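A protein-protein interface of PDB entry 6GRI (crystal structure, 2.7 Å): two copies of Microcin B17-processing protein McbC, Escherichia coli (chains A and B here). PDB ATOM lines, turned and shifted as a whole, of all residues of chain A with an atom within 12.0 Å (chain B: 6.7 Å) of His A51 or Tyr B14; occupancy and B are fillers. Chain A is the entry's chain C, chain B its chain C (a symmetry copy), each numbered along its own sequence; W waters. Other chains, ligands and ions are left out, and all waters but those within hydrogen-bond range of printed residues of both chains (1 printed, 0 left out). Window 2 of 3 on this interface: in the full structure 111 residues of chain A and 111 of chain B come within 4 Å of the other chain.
O of Lys B201 sits at hydrogen-bond distance from N of Ala A46 (3.0 Å). OH of Tyr B14 lies within hydrogen-bond range of ND1 of His A51 (3.5 Å). The side-chain amino group (NZ) of Lys A54 lies within salt-bridge range of the side-chain carboxylate (OE1) of Glu B10, 3.7 Å away. The backbone carbonyl oxygen (O) of Val A44 lies close to the backbone carbonyl oxygen (O) of Lys B201 (3.3 Å).
No position is printed for both chains.
Of the printed residues of chain B, Ser A45 touches Lys B201 (3.2 Å). Of chain B, only Tyr B14 comes within 4 Å of His A51. Of the printed residues of chain B, Lys A54 touches Glu B10. Glu A56 touches none of the printed residues of chain B. Val B9 touches none of the printed residues of chain A. Of the printed residues of chain A, Val B11 touches Phe A55. No residue of chain A comes within 4 Å of Thr B12. No residue of chain A comes within 4 Å of His B13. Tyr B14 touches five residues of chain A. No residue of chain A comes within 4 Å of Thr B15. No residue of chain A comes within 4 Å of Asp B16. Phe B200 touches just these residues of chain A: Ala A46, Val A47 and Phe A55. Printed residues of chain A within 4 Å of Lys B201: Val A44 (3.3 Å), Ser A45 (3.2 Å), Ala A46 (3.0 Å) and Leu A52 (3.6 Å). The nearest printed residue of chain B that does not touch Val A47 is Lys B201 (4.5 Å).
OG of Ser A45 is in hydrogen-bond range of O of Val A47.
Water W1 bridges the side-chain carboxylate of Glu A56 (2.7 Å) and the side-chain amino group of Lys B201 (2.8 Å).
Along chain B the printed residues that touch a printed residue of chain A span positions 10 to 201. Of the 16 printed residues of chain A, 9 touch a printed residue of chain B. Printed residues of chain A that touch a printed residue of chain B: Val A44, Ser A45, Ala A46, Val A47, Pro A48, His A51, Leu A52, Lys A54 and Phe A55.
Among the printed residues, merely in contact across the chains: Ser A45 with Lys B201, Ala A46 with Phe B200, Pro A48 with Tyr B14, Phe A55 with Phe B200, Ala A46 with Tyr B14, Leu A52 with Lys B201, Val A47 with Tyr B14, Phe A55 with Glu B10, Phe A55 with Val B11, Val A47 with Phe B200 and Phe A55 with Tyr B14.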
ATOM      1  N   PHE A  43      -3.767  32.923   4.188  1.00  0.00           N
ATOM      2  CA  PHE A  43      -3.220  32.642   5.507  1.00  0.00           C
ATOM      3  C   PHE A  43      -1.790  33.140   5.588  1.00  0.00           C
ATOM      4  O   PHE A  43      -1.177  33.446   4.570  1.00  0.00           O
ATOM      5  CB  PHE A  43      -3.305  31.159   5.830  1.00  0.00           C
ATOM      6  CG  PHE A  43      -2.449  30.296   4.958  1.00  0.00           C
ATOM      7  CD1 PHE A  43      -2.880  29.917   3.702  1.00  0.00           C
ATOM      8  CD2 PHE A  43      -1.216  29.844   5.406  1.00  0.00           C
ATOM      9  CE1 PHE A  43      -2.091  29.119   2.894  1.00  0.00           C
ATOM     10  CE2 PHE A  43      -0.425  29.053   4.608  1.00  0.00           C
ATOM     11  CZ  PHE A  43      -0.864  28.692   3.346  1.00  0.00           C
ATOM     12  N   VAL A  44      -1.284  33.242   6.810  1.00  0.00           N
ATOM     13  CA  VAL A  44       0.096  33.629   7.062  1.00  0.00           C
ATOM     14  C   VAL A  44       0.971  32.437   7.490  1.00  0.00           C
ATOM     15  O   VAL A  44       2.048  32.245   6.924  1.00  0.00           O
ATOM     16  CB  VAL A  44       0.145  34.747   8.113  1.00  0.00           C
ATOM     17  CG1 VAL A  44       1.573  34.996   8.599  1.00  0.00           C
ATOM     18  CG2 VAL A  44      -0.440  36.012   7.515  1.00  0.00           C
ATOM     19  N   SER A  45       0.517  31.664   8.487  1.00  0.00           N
ATOM     20  CA  SER A  45       1.306  30.549   9.052  1.00  0.00           C
ATOM     21  C   SER A  45       1.129  29.220   8.311  1.00  0.00           C
ATOM     22  O   SER A  45       0.016  28.731   8.163  1.00  0.00           O
ATOM     23  CB  SER A  45       0.952  30.317  10.521  1.00  0.00           C
ATOM     24  OG  SER A  45       1.679  29.213  11.039  1.00  0.00           O
ATOM     25  N   ALA A  46       2.241  28.626   7.894  1.00  0.00           N
ATOM     26  CA  ALA A  46       2.249  27.277   7.326  1.00  0.00           C
ATOM     27  C   ALA A  46       1.950  26.174   8.353  1.00  0.00           C
ATOM     28  O   ALA A  46       1.502  25.095   7.967  1.00  0.00           O
ATOM     29  CB  ALA A  46       3.581  27.013   6.663  1.00  0.00           C
ATOM     30  N   VAL A  47       2.207  26.445   9.640  1.00  0.00           N
ATOM     31  CA  VAL A  47       1.912  25.514  10.733  1.00  0.00           C
ATOM     32  C   VAL A  47       0.531  25.852  11.291  1.00  0.00           C
ATOM     33  O   VAL A  47       0.293  27.002  11.642  1.00  0.00           O
ATOM     34  CB  VAL A  47       2.921  25.641  11.905  1.00  0.00           C
ATOM     35  CG1 VAL A  47       2.641  24.566  12.962  1.00  0.00           C
ATOM     36  CG2 VAL A  47       4.362  25.567  11.413  1.00  0.00           C
ATOM     37  N   PRO A  48      -0.373  24.861  11.411  1.00  0.00           N
ATOM     38  CA  PRO A  48      -1.683  25.112  12.026  1.00  0.00           C
ATOM     39  C   PRO A  48      -1.617  25.655  13.452  1.00  0.00           C
ATOM     40  O   PRO A  48      -0.663  25.361  14.180  1.00  0.00           O
ATOM     41  CB  PRO A  48      -2.334  23.729  12.049  1.00  0.00           C
ATOM     42  CG  PRO A  48      -1.671  22.973  10.962  1.00  0.00           C
ATOM     43  CD  PRO A  48      -0.268  23.483  10.905  1.00  0.00           C
ATOM     44  N   LEU A  49      -2.639  26.430  13.826  1.00  0.00           N
ATOM     45  CA  LEU A  49      -2.777  27.002  15.167  1.00  0.00           C
ATOM     46  C   LEU A  49      -2.527  25.968  16.267  1.00  0.00           C
ATOM     47  O   LEU A  49      -1.766  26.232  17.194  1.00  0.00           O
ATOM     48  CB  LEU A  49      -4.182  27.600  15.337  1.00  0.00           C
ATOM     49  CG  LEU A  49      -4.603  28.073  16.744  1.00  0.00           C
ATOM     50  CD1 LEU A  49      -3.793  29.304  17.145  1.00  0.00           C
ATOM     51  CD2 LEU A  49      -6.102  28.340  16.829  1.00  0.00           C
ATOM     52  N   ALA A  50      -3.189  24.813  16.164  1.00  0.00           N
ATOM     53  CA  ALA A  50      -3.011  23.693  17.111  1.00  0.00           C
ATOM     54  C   ALA A  50      -1.558  23.460  17.500  1.00  0.00           C
ATOM     55  O   ALA A  50      -1.193  23.560  18.671  1.00  0.00           O
ATOM     56  CB  ALA A  50      -3.582  22.407  16.522  1.00  0.00           C
ATOM     57  N   HIS A  51      -0.728  23.203  16.494  1.00  0.00           N
ATOM     58  CA  HIS A  51       0.635  22.714  16.698  1.00  0.00           C
ATOM     59  C   HIS A  51       1.695  23.792  16.958  1.00  0.00           C
ATOM     60  O   HIS A  51       2.863  23.451  17.123  1.00  0.00           O
ATOM     61  CB  HIS A  51       1.057  21.874  15.488  1.00  0.00           C
ATOM     62  CG  HIS A  51       0.139  20.724  15.194  1.00  0.00           C
ATOM     63  ND1 HIS A  51      -0.698  20.701  14.098  1.00  0.00           N
ATOM     64  CD2 HIS A  51      -0.070  19.557  15.853  1.00  0.00           C
ATOM     65  CE1 HIS A  51      -1.380  19.569  14.093  1.00  0.00           C
ATOM     66  NE2 HIS A  51      -1.017  18.858  15.146  1.00  0.00           N
ATOM     67  N   LEU A  52       1.310  25.070  17.014  1.00  0.00           N
ATOM     68  CA  LEU A  52       2.290  26.174  17.082  1.00  0.00           C
ATOM     69  C   LEU A  52       3.085  26.242  18.390  1.00  0.00           C
ATOM     70  O   LEU A  52       4.275  26.542  18.359  1.00  0.00           O
ATOM     71  CB  LEU A  52       1.634  27.547  16.809  1.00  0.00           C
ATOM     72  CG  LEU A  52       1.604  28.083  15.372  1.00  0.00           C
ATOM     73  CD1 LEU A  52       0.688  29.286  15.274  1.00  0.00           C
ATOM     74  CD2 LEU A  52       2.984  28.481  14.874  1.00  0.00           C
ATOM     75  N   GLU A  53       2.443  25.962  19.522  1.00  0.00           N
ATOM     76  CA  GLU A  53       3.088  26.104  20.841  1.00  0.00           C
ATOM     77  C   GLU A  53       4.259  25.128  21.059  1.00  0.00           C
ATOM     78  O   GLU A  53       5.129  25.359  21.881  1.00  0.00           O
ATOM     79  CB  GLU A  53       2.041  25.970  21.949  1.00  0.00           C
ATOM     80  CG  GLU A  53       2.556  26.241  23.355  1.00  0.00           C
ATOM     81  CD  GLU A  53       2.810  24.968  24.138  1.00  0.00           C
ATOM     82  OE1 GLU A  53       1.811  24.326  24.521  1.00  0.00           O
ATOM     83  OE2 GLU A  53       3.988  24.607  24.373  1.00  0.00           O
ATOM     84  N   LYS A  54       4.265  24.042  20.303  1.00  0.00           N
ATOM     85  CA  LYS A  54       5.399  23.140  20.216  1.00  0.00           C
ATOM     86  C   LYS A  54       6.691  23.836  19.754  1.00  0.00           C
ATOM     87  O   LYS A  54       7.772  23.434  20.169  1.00  0.00           O
ATOM     88  CB  LYS A  54       5.025  22.025  19.247  1.00  0.00           C
ATOM     89  CG  LYS A  54       5.963  20.826  19.167  1.00  0.00           C
ATOM     90  CD  LYS A  54       5.704  20.021  17.897  1.00  0.00           C
ATOM     91  CE  LYS A  54       4.279  19.462  17.806  1.00  0.00           C
ATOM     92  NZ  LYS A  54       3.686  19.585  16.443  1.00  0.00           N
ATOM     93  N   PHE A  55       6.585  24.870  18.917  1.00  0.00           N
ATOM     94  CA  PHE A  55       7.755  25.561  18.321  1.00  0.00           C
ATOM     95  C   PHE A  55       8.171  26.889  18.971  1.00  0.00           C
ATOM     96  O   PHE A  55       9.250  27.418  18.690  1.00  0.00           O
ATOM     97  CB  PHE A  55       7.475  25.792  16.847  1.00  0.00           C
ATOM     98  CG  PHE A  55       7.143  24.535  16.115  1.00  0.00           C
ATOM     99  CD1 PHE A  55       8.151  23.724  15.614  1.00  0.00           C
ATOM    100  CD2 PHE A  55       5.827  24.125  15.972  1.00  0.00           C
ATOM    101  CE1 PHE A  55       7.848  22.551  14.949  1.00  0.00           C
ATOM    102  CE2 PHE A  55       5.519  22.946  15.317  1.00  0.00           C
ATOM    103  CZ  PHE A  55       6.527  22.160  14.801  1.00  0.00           C
ATOM    104  N   GLU A  56       7.326  27.401  19.858  1.00  0.00           N
ATOM    105  CA  GLU A  56       7.502  28.723  20.454  1.00  0.00           C
ATOM    106  C   GLU A  56       8.341  28.682  21.715  1.00  0.00           C
ATOM    107  O   GLU A  56       8.102  27.877  22.597  1.00  0.00           O
ATOM    108  CB  GLU A  56       6.131  29.337  20.749  1.00  0.00           C
ATOM    109  CG  GLU A  56       5.353  29.582  19.461  1.00  0.00           C
ATOM    110  CD  GLU A  56       3.884  29.882  19.647  1.00  0.00           C
ATOM    111  OE1 GLU A  56       3.377  29.824  20.784  1.00  0.00           O
ATOM    112  OE2 GLU A  56       3.230  30.179  18.623  1.00  0.00           O
ATOM    113  N   ASN A  57       9.333  29.561  21.770  1.00  0.00           N
ATOM    114  CA  ASN A  57      10.187  29.758  22.945  1.00  0.00           C
ATOM    115  C   ASN A  57      10.917  28.499  23.386  1.00  0.00           C
ATOM    116  O   ASN A  57      10.790  28.049  24.525  1.00  0.00           O
ATOM    117  CB  ASN A  57       9.392  30.393  24.097  1.00  0.00           C
ATOM    118  CG  ASN A  57       9.162  31.864  23.884  1.00  0.00           C
ATOM    119  OD1 ASN A  57      10.116  32.651  23.861  1.00  0.00           O
ATOM    120  ND2 ASN A  57       7.902  32.250  23.714  1.00  0.00           N
ATOM    121  N   LYS A  58      11.706  27.972  22.458  1.00  0.00           N
ATOM    122  CA  LYS A  58      12.458  26.751  22.651  1.00  0.00           C
ATOM    123  C   LYS A  58      13.907  26.955  22.276  1.00  0.00           C
ATOM    124  O   LYS A  58      14.255  27.925  21.615  1.00  0.00           O
ATOM    125  CB  LYS A  58      11.900  25.660  21.753  1.00  0.00           C
ATOM    126  CG  LYS A  58      10.402  25.469  21.838  1.00  0.00           C
ATOM    127  CD  LYS A  58       9.966  24.999  23.210  1.00  0.00           C
ATOM    128  CE  LYS A  58       8.557  24.458  23.132  1.00  0.00           C
ATOM    129  NZ  LYS A  58       8.004  24.157  24.475  1.00  0.00           N
ATOM    130  N   VAL B   9      13.481  17.930  13.603  1.00  0.00           N
ATOM    131  CA  VAL B   9      12.662  16.959  12.862  1.00  0.00           C
ATOM    132  C   VAL B   9      11.189  17.400  12.861  1.00  0.00           C
ATOM    133  O   VAL B   9      10.465  17.151  11.899  1.00  0.00           O
ATOM    134  CB  VAL B   9      12.714  15.538  13.485  1.00  0.00           C
ATOM    135  CG1 VAL B   9      11.939  14.542  12.627  1.00  0.00           C
ATOM    136  CG2 VAL B   9      14.140  15.031  13.672  1.00  0.00           C
ATOM    137  N   GLU B  10      10.748  18.009  13.968  1.00  0.00           N
ATOM    138  CA  GLU B  10       9.416  18.610  14.065  1.00  0.00           C
ATOM    139  C   GLU B  10       9.303  19.809  13.113  1.00  0.00           C
ATOM    140  O   GLU B  10       8.289  19.965  12.436  1.00  0.00           O
ATOM    141  CB  GLU B  10       9.122  19.076  15.489  1.00  0.00           C
ATOM    142  CG  GLU B  10       9.098  17.994  16.550  1.00  0.00           C
ATOM    143  CD  GLU B  10       7.854  17.123  16.516  1.00  0.00           C
ATOM    144  OE1 GLU B  10       6.772  17.595  16.123  1.00  0.00           O
ATOM    145  OE2 GLU B  10       7.955  15.944  16.911  1.00  0.00           O
ATOM    146  N   VAL B  11      10.339  20.650  13.080  1.00  0.00           N
ATOM    147  CA  VAL B  11      10.388  21.792  12.174  1.00  0.00           C
ATOM    148  C   VAL B  11      10.279  21.315  10.724  1.00  0.00           C
ATOM    149  O   VAL B  11       9.388  21.754  10.000  1.00  0.00           O
ATOM    150  CB  VAL B  11      11.661  22.663  12.399  1.00  0.00           C
ATOM    151  CG1 VAL B  11      11.894  23.647  11.253  1.00  0.00           C
ATOM    152  CG2 VAL B  11      11.565  23.418  13.723  1.00  0.00           C
ATOM    153  N   THR B  12      11.139  20.377  10.335  1.00  0.00           N
ATOM    154  CA  THR B  12      11.239  19.933   8.942  1.00  0.00           C
ATOM    155  C   THR B  12       9.977  19.321   8.335  1.00  0.00           C
ATOM    156  O   THR B  12       9.903  19.168   7.129  1.00  0.00           O
ATOM    157  CB  THR B  12      12.422  18.973   8.719  1.00  0.00           C
ATOM    158  OG1 THR B  12      12.916  19.133   7.386  1.00  0.00           O
ATOM    159  CG2 THR B  12      12.037  17.492   8.945  1.00  0.00           C
ATOM    160  N   HIS B  13       9.001  18.973   9.160  1.00  0.00           N
ATOM    161  CA  HIS B  13       7.683  18.534   8.695  1.00  0.00           C
ATOM    162  C   HIS B  13       6.895  19.603   7.893  1.00  0.00           C
ATOM    163  O   HIS B  13       6.047  19.249   7.090  1.00  0.00           O
ATOM    164  CB  HIS B  13       6.880  18.060   9.921  1.00  0.00           C
ATOM    165  CG  HIS B  13       5.530  17.498   9.607  1.00  0.00           C
ATOM    166  ND1 HIS B  13       5.329  16.165   9.314  1.00  0.00           N
ATOM    167  CD2 HIS B  13       4.309  18.083   9.567  1.00  0.00           C
ATOM    168  CE1 HIS B  13       4.042  15.958   9.093  1.00  0.00           C
ATOM    169  NE2 HIS B  13       3.400  17.105   9.236  1.00  0.00           N
ATOM    170  N   TYR B  14       7.166  20.890   8.118  1.00  0.00           N
ATOM    171  CA  TYR B  14       6.443  21.992   7.462  1.00  0.00           C
ATOM    172  C   TYR B  14       7.284  22.725   6.413  1.00  0.00           C
ATOM    173  O   TYR B  14       6.903  23.804   5.954  1.00  0.00           O
ATOM    174  CB  TYR B  14       5.985  23.009   8.515  1.00  0.00           C
ATOM    175  CG  TYR B  14       4.979  22.459   9.490  1.00  0.00           C
ATOM    176  CD1 TYR B  14       3.618  22.550   9.225  1.00  0.00           C
ATOM    177  CD2 TYR B  14       5.383  21.845  10.687  1.00  0.00           C
ATOM    178  CE1 TYR B  14       2.689  22.045  10.110  1.00  0.00           C
ATOM    179  CE2 TYR B  14       4.452  21.338  11.577  1.00  0.00           C
ATOM    180  CZ  TYR B  14       3.111  21.436  11.278  1.00  0.00           C
ATOM    181  OH  TYR B  14       2.167  20.942  12.133  1.00  0.00           O
ATOM    182  N   THR B  15       8.417  22.155   6.028  1.00  0.00           N
ATOM    183  CA  THR B  15       9.355  22.853   5.168  1.00  0.00           C
ATOM    184  C   THR B  15       8.956  22.753   3.719  1.00  0.00           C
ATOM    185  O   THR B  15       8.796  21.659   3.188  1.00  0.00           O
ATOM    186  CB  THR B  15      10.764  22.273   5.316  1.00  0.00           C
ATOM    187  OG1 THR B  15      11.200  22.476   6.660  1.00  0.00           O
ATOM    188  CG2 THR B  15      11.755  22.940   4.328  1.00  0.00           C
ATOM    189  N   ASP B  16       8.816  23.901   3.074  1.00  0.00           N
ATOM    190  CA  ASP B  16       8.684  23.943   1.626  1.00  0.00           C
ATOM    191  C   ASP B  16      10.096  23.877   1.053  1.00  0.00           C
ATOM    192  O   ASP B  16      10.914  24.766   1.308  1.00  0.00           O
ATOM    193  CB  ASP B  16       7.972  25.217   1.168  1.00  0.00           C
ATOM    194  CG  ASP B  16       7.654  25.201  -0.305  1.00  0.00           C
ATOM    195  OD1 ASP B  16       8.444  24.637  -1.090  1.00  0.00           O
ATOM    196  OD2 ASP B  16       6.609  25.758  -0.679  1.00  0.00           O
ATOM    197  N   GLU B 196      15.843  26.190   8.037  1.00  0.00           N
ATOM    198  CA  GLU B 196      14.523  25.543   8.116  1.00  0.00           C
ATOM    199  C   GLU B 196      13.627  26.069   9.249  1.00  0.00           C
ATOM    200  O   GLU B 196      12.405  26.137   9.089  1.00  0.00           O
ATOM    201  CB  GLU B 196      14.664  24.020   8.195  1.00  0.00           C
ATOM    202  CG  GLU B 196      15.240  23.408   6.913  1.00  0.00           C
ATOM    203  CD  GLU B 196      14.771  21.982   6.641  1.00  0.00           C
ATOM    204  OE1 GLU B 196      13.583  21.664   6.856  1.00  0.00           O
ATOM    205  OE2 GLU B 196      15.606  21.171   6.190  1.00  0.00           O
ATOM    206  N   LEU B 199      12.335  29.521   8.042  1.00  0.00           N
ATOM    207  CA  LEU B 199      11.415  29.532   6.899  1.00  0.00           C
ATOM    208  C   LEU B 199      10.084  28.779   7.067  1.00  0.00           C
ATOM    209  O   LEU B 199       9.130  29.022   6.304  1.00  0.00           O
ATOM    210  CB  LEU B 199      12.157  28.998   5.670  1.00  0.00           C
ATOM    211  CG  LEU B 199      13.383  29.817   5.245  1.00  0.00           C
ATOM    212  CD1 LEU B 199      14.249  29.003   4.301  1.00  0.00           C
ATOM    213  CD2 LEU B 199      12.981  31.148   4.610  1.00  0.00           C
ATOM    214  N   PHE B 200      10.015  27.863   8.031  1.00  0.00           N
ATOM    215  CA  PHE B 200       8.879  26.916   8.098  1.00  0.00           C
ATOM    216  C   PHE B 200       7.488  27.497   8.376  1.00  0.00           C
ATOM    217  O   PHE B 200       6.503  26.913   7.955  1.00  0.00           O
ATOM    218  CB  PHE B 200       9.169  25.708   9.023  1.00  0.00           C
ATOM    219  CG  PHE B 200       8.973  25.970  10.501  1.00  0.00           C
ATOM    220  CD1 PHE B 200       9.684  26.969  11.161  1.00  0.00           C
ATOM    221  CD2 PHE B 200       8.113  25.161  11.248  1.00  0.00           C
ATOM    222  CE1 PHE B 200       9.510  27.172  12.520  1.00  0.00           C
ATOM    223  CE2 PHE B 200       7.939  25.363  12.608  1.00  0.00           C
ATOM    224  CZ  PHE B 200       8.634  26.368  13.248  1.00  0.00           C
ATOM    225  N   LYS B 201       7.408  28.626   9.066  1.00  0.00           N
ATOM    226  CA  LYS B 201       6.116  29.259   9.354  1.00  0.00           C
ATOM    227  C   LYS B 201       5.766  30.398   8.362  1.00  0.00           C
ATOM    228  O   LYS B 201       4.666  30.430   7.813  1.00  0.00           O
ATOM    229  CB  LYS B 201       6.114  29.791  10.783  1.00  0.00           C
ATOM    230  CG  LYS B 201       4.726  30.100  11.294  1.00  0.00           C
ATOM    231  CD  LYS B 201       4.749  30.779  12.651  1.00  0.00           C
ATOM    232  CE  LYS B 201       3.408  31.441  12.946  1.00  0.00           C
ATOM    233  NZ  LYS B 201       3.417  32.243  14.197  1.00  0.00           N
HETATM  234  O   HOH W   1       4.566  31.056  16.452  1.00  0.00           O
